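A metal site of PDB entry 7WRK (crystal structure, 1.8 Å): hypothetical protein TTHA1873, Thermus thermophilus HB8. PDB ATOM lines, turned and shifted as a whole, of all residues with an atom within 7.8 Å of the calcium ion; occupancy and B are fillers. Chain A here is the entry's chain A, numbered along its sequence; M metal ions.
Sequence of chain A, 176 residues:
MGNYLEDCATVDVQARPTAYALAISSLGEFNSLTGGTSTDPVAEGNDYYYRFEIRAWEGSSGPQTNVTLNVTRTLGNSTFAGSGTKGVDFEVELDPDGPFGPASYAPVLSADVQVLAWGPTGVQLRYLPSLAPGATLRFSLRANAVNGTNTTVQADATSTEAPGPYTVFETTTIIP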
ATOM      1  N   SER A  26     -34.647 -13.670   0.700  1.00  0.00           N
ATOM      2  CA  SER A  26     -34.307 -14.494   1.864  1.00  0.00           C
ATOM      3  C   SER A  26     -35.376 -14.351   2.924  1.00  0.00           C
ATOM      4  O   SER A  26     -35.832 -13.212   3.148  1.00  0.00           O
ATOM      5  CB  SER A  26     -32.958 -14.106   2.426  1.00  0.00           C
ATOM      6  OG  SER A  26     -32.634 -15.029   3.477  1.00  0.00           O
ATOM      7  N   LEU A  27     -35.739 -15.443   3.604  1.00  0.00           N
ATOM      8  CA  LEU A  27     -36.662 -15.420   4.768  1.00  0.00           C
ATOM      9  C   LEU A  27     -35.901 -15.753   6.069  1.00  0.00           C
ATOM     10  O   LEU A  27     -36.504 -15.780   7.096  1.00  0.00           O
ATOM     11  CB  LEU A  27     -37.775 -16.449   4.537  1.00  0.00           C
ATOM     12  CG  LEU A  27     -38.564 -16.349   3.238  1.00  0.00           C
ATOM     13  CD1 LEU A  27     -39.702 -17.356   3.204  1.00  0.00           C
ATOM     14  CD2 LEU A  27     -39.105 -14.949   3.027  1.00  0.00           C
ATOM     15  N   GLY A  28     -34.616 -16.006   5.965  1.00  0.00           N
ATOM     16  CA  GLY A  28     -33.793 -16.391   7.104  1.00  0.00           C
ATOM     17  C   GLY A  28     -33.924 -17.860   7.461  1.00  0.00           C
ATOM     18  O   GLY A  28     -34.419 -18.662   6.684  1.00  0.00           O
ATOM     19  N   GLU A  29     -33.447 -18.176   8.641  1.00  0.00           N
ATOM     20  CA  GLU A  29     -33.286 -19.551   9.140  1.00  0.00           C
ATOM     21  C   GLU A  29     -34.462 -19.933  10.053  1.00  0.00           C
ATOM     22  O   GLU A  29     -34.986 -19.065  10.774  1.00  0.00           O
ATOM     23  CB  GLU A  29     -31.970 -19.701   9.911  1.00  0.00           C
ATOM     24  CG  GLU A  29     -30.742 -19.386   9.075  1.00  0.00           C
ATOM     25  CD  GLU A  29     -30.342 -17.916   9.037  1.00  0.00           C
ATOM     26  OE1 GLU A  29     -31.110 -17.062   9.570  1.00  0.00           O
ATOM     27  OE2 GLU A  29     -29.225 -17.632   8.597  1.00  0.00           O
ATOM     28  N   THR A  39     -34.814 -19.274  13.811  1.00  0.00           N
ATOM     29  CA  THR A  39     -33.573 -19.448  14.582  1.00  0.00           C
ATOM     30  C   THR A  39     -32.480 -18.572  13.968  1.00  0.00           C
ATOM     31  O   THR A  39     -32.832 -17.756  13.166  1.00  0.00           O
ATOM     32  CB  THR A  39     -33.218 -20.939  14.677  1.00  0.00           C
ATOM     33  OG1 THR A  39     -32.165 -21.131  15.614  1.00  0.00           O
ATOM     34  CG2 THR A  39     -32.822 -21.579  13.397  1.00  0.00           C
ATOM     35  N   ASP A  40     -31.229 -18.790  14.400  1.00  0.00           N
ATOM     36  CA  ASP A  40     -30.044 -17.957  14.152  1.00  0.00           C
ATOM     37  C   ASP A  40     -29.891 -17.002  15.339  1.00  0.00           C
ATOM     38  O   ASP A  40     -30.760 -16.156  15.585  1.00  0.00           O
ATOM     39  CB  ASP A  40     -30.104 -17.143  12.868  1.00  0.00           C
ATOM     40  CG  ASP A  40     -28.738 -16.684  12.377  1.00  0.00           C
ATOM     41  OD1 ASP A  40     -27.738 -17.131  12.967  1.00  0.00           O
ATOM     42  OD2 ASP A  40     -28.738 -15.883  11.383  1.00  0.00           O
ATOM     43  N   PRO A  41     -28.800 -17.115  16.121  1.00  0.00           N
ATOM     44  CA  PRO A  41     -27.764 -18.121  15.939  1.00  0.00           C
ATOM     45  C   PRO A  41     -28.145 -19.600  16.065  1.00  0.00           C
ATOM     46  O   PRO A  41     -29.266 -19.883  16.548  1.00  0.00           O
ATOM     47  CB  PRO A  41     -26.800 -17.877  17.105  1.00  0.00           C
ATOM     48  CG  PRO A  41     -26.970 -16.412  17.393  1.00  0.00           C
ATOM     49  CD  PRO A  41     -28.464 -16.170  17.185  1.00  0.00           C
ATOM     50  N   TYR A  48     -30.488 -26.968  11.067  1.00  0.00           N
ATOM     51  CA  TYR A  48     -31.336 -25.758  10.879  1.00  0.00           C
ATOM     52  C   TYR A  48     -31.736 -25.681   9.414  1.00  0.00           C
ATOM     53  O   TYR A  48     -31.261 -26.505   8.595  1.00  0.00           O
ATOM     54  CB  TYR A  48     -30.628 -24.487  11.339  1.00  0.00           C
ATOM     55  CG  TYR A  48     -29.454 -24.067  10.489  1.00  0.00           C
ATOM     56  CD1 TYR A  48     -28.202 -24.624  10.666  1.00  0.00           C
ATOM     57  CD2 TYR A  48     -29.569 -23.046   9.570  1.00  0.00           C
ATOM     58  CE1 TYR A  48     -27.112 -24.225   9.915  1.00  0.00           C
ATOM     59  CE2 TYR A  48     -28.486 -22.644   8.789  1.00  0.00           C
ATOM     60  CZ  TYR A  48     -27.241 -23.214   8.981  1.00  0.00           C
ATOM     61  OH  TYR A  48     -26.146 -22.832   8.216  1.00  0.00           O
ATOM     62  N   TYR A  50     -32.573 -23.105   5.902  1.00  0.00           N
ATOM     63  CA  TYR A  50     -32.676 -21.810   5.184  1.00  0.00           C
ATOM     64  C   TYR A  50     -34.039 -21.841   4.469  1.00  0.00           C
ATOM     65  O   TYR A  50     -34.391 -22.895   3.933  1.00  0.00           O
ATOM     66  CB  TYR A  50     -31.589 -21.664   4.125  1.00  0.00           C
ATOM     67  CG  TYR A  50     -30.217 -21.407   4.693  1.00  0.00           C
ATOM     68  CD1 TYR A  50     -29.894 -20.166   5.200  1.00  0.00           C
ATOM     69  CD2 TYR A  50     -29.305 -22.451   4.805  1.00  0.00           C
ATOM     70  CE1 TYR A  50     -28.659 -19.922   5.775  1.00  0.00           C
ATOM     71  CE2 TYR A  50     -28.056 -22.213   5.339  1.00  0.00           C
ATOM     72  CZ  TYR A  50     -27.722 -20.945   5.832  1.00  0.00           C
ATOM     73  OH  TYR A  50     -26.532 -20.699   6.445  1.00  0.00           O
ATOM     74  N   THR A 151     -21.567 -18.784   8.732  1.00  0.00           N
ATOM     75  CA  THR A 151     -21.861 -19.399   7.416  1.00  0.00           C
ATOM     76  C   THR A 151     -22.652 -18.398   6.557  1.00  0.00           C
ATOM     77  O   THR A 151     -23.659 -17.859   7.031  1.00  0.00           O
ATOM     78  CB  THR A 151     -22.624 -20.702   7.520  1.00  0.00           C
ATOM     79  OG1 THR A 151     -21.809 -21.664   8.210  1.00  0.00           O
ATOM     80  CG2 THR A 151     -23.045 -21.167   6.138  1.00  0.00           C
ATOM     81  N   PHE A 169     -27.800 -13.023  -0.366  1.00  0.00           N
ATOM     82  CA  PHE A 169     -26.860 -13.695   0.536  1.00  0.00           C
ATOM     83  C   PHE A 169     -27.490 -13.687   1.929  1.00  0.00           C
ATOM     84  O   PHE A 169     -27.759 -12.567   2.443  1.00  0.00           O
ATOM     85  CB  PHE A 169     -25.499 -13.005   0.530  1.00  0.00           C
ATOM     86  CG  PHE A 169     -24.688 -13.096  -0.750  1.00  0.00           C
ATOM     87  CD1 PHE A 169     -24.958 -12.262  -1.829  1.00  0.00           C
ATOM     88  CD2 PHE A 169     -23.623 -13.984  -0.868  1.00  0.00           C
ATOM     89  CE1 PHE A 169     -24.185 -12.279  -2.987  1.00  0.00           C
ATOM     90  CE2 PHE A 169     -22.860 -14.027  -2.026  1.00  0.00           C
ATOM     91  CZ  PHE A 169     -23.148 -13.179  -3.086  1.00  0.00           C
ATOM     92  N   GLU A 170     -27.551 -14.853   2.556  1.00  0.00           N
ATOM     93  CA  GLU A 170     -28.043 -14.990   3.938  1.00  0.00           C
ATOM     94  C   GLU A 170     -26.919 -15.568   4.786  1.00  0.00           C
ATOM     95  O   GLU A 170     -26.124 -16.373   4.282  1.00  0.00           O
ATOM     96  CB  GLU A 170     -29.262 -15.906   3.993  1.00  0.00           C
ATOM     97  CG  GLU A 170     -29.831 -15.990   5.387  1.00  0.00           C
ATOM     98  CD  GLU A 170     -30.360 -14.723   6.041  1.00  0.00           C
ATOM     99  OE1 GLU A 170     -31.204 -14.018   5.461  1.00  0.00           O
ATOM    100  OE2 GLU A 170     -29.923 -14.474   7.189  1.00  0.00           O
ATOM    101  N   THR A 171     -26.852 -15.158   6.048  1.00  0.00           N
ATOM    102  CA  THR A 171     -25.714 -15.422   6.931  1.00  0.00           C
ATOM    103  C   THR A 171     -26.264 -15.938   8.253  1.00  0.00           C
ATOM    104  O   THR A 171     -27.197 -15.368   8.762  1.00  0.00           O
ATOM    105  CB  THR A 171     -24.842 -14.189   7.146  1.00  0.00           C
ATOM    106  OG1 THR A 171     -24.320 -13.760   5.860  1.00  0.00           O
ATOM    107  CG2 THR A 171     -23.665 -14.461   8.041  1.00  0.00           C
ATOM    108  N   THR A 172     -25.601 -16.974   8.773  1.00  0.00           N
ATOM    109  CA  THR A 172     -25.977 -17.680   9.989  1.00  0.00           C
ATOM    110  C   THR A 172     -24.791 -17.644  10.941  1.00  0.00           C
ATOM    111  O   THR A 172     -23.657 -17.924  10.552  1.00  0.00           O
ATOM    112  CB  THR A 172     -26.365 -19.135   9.687  1.00  0.00           C
ATOM    113  OG1 THR A 172     -27.158 -19.203   8.492  1.00  0.00           O
ATOM    114  CG2 THR A 172     -27.118 -19.713  10.855  1.00  0.00           C
ATOM    115  N   THR A 173     -25.072 -17.224  12.147  1.00  0.00           N
ATOM    116  CA  THR A 173     -24.103 -17.172  13.254  1.00  0.00           C
ATOM    117  C   THR A 173     -24.069 -18.552  13.903  1.00  0.00           C
ATOM    118  O   THR A 173     -25.131 -19.017  14.275  1.00  0.00           O
ATOM    119  CB  THR A 173     -24.473 -16.111  14.271  1.00  0.00           C
ATOM    120  OG1 THR A 173     -24.479 -14.857  13.592  1.00  0.00           O
ATOM    121  CG2 THR A 173     -23.472 -16.088  15.382  1.00  0.00           C
HETATM  122 CA    CA M   1     -29.483 -15.233   9.343  1.00  0.00          CA
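Four residues have an atom within 4 Å of the calcium ion: Glu 29, Asp 40, Glu 170 and Thr 171. Along chain A the residues within 4 Å of the calcium ion span positions 29 to 171.
The calcium ion is bound by OD2 of Asp 40 (2.3 Å), OE2 of Glu 170 (2.3 Å), O of Thr 171 (2.4 Å), OE1 of Glu 29 (2.5 Å) and OE2 of Glu 29 (2.5 Å).
The side-chain carboxylate (OE1) of Glu 170 lies within hydrogen-bond range of the side-chain hydroxyl (OG) of Ser 26 (2.6 Å). The side-chain carboxylate (OE2) of Glu 29 sits close to the side-chain hydroxyl (OG1) of Thr 172 (2.6 Å). N of Thr 173 lies within hydrogen-bond range of OD1 of Asp 40. O of Glu 29 sits at hydrogen-bond distance from N of Thr 39 (3.0 Å).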
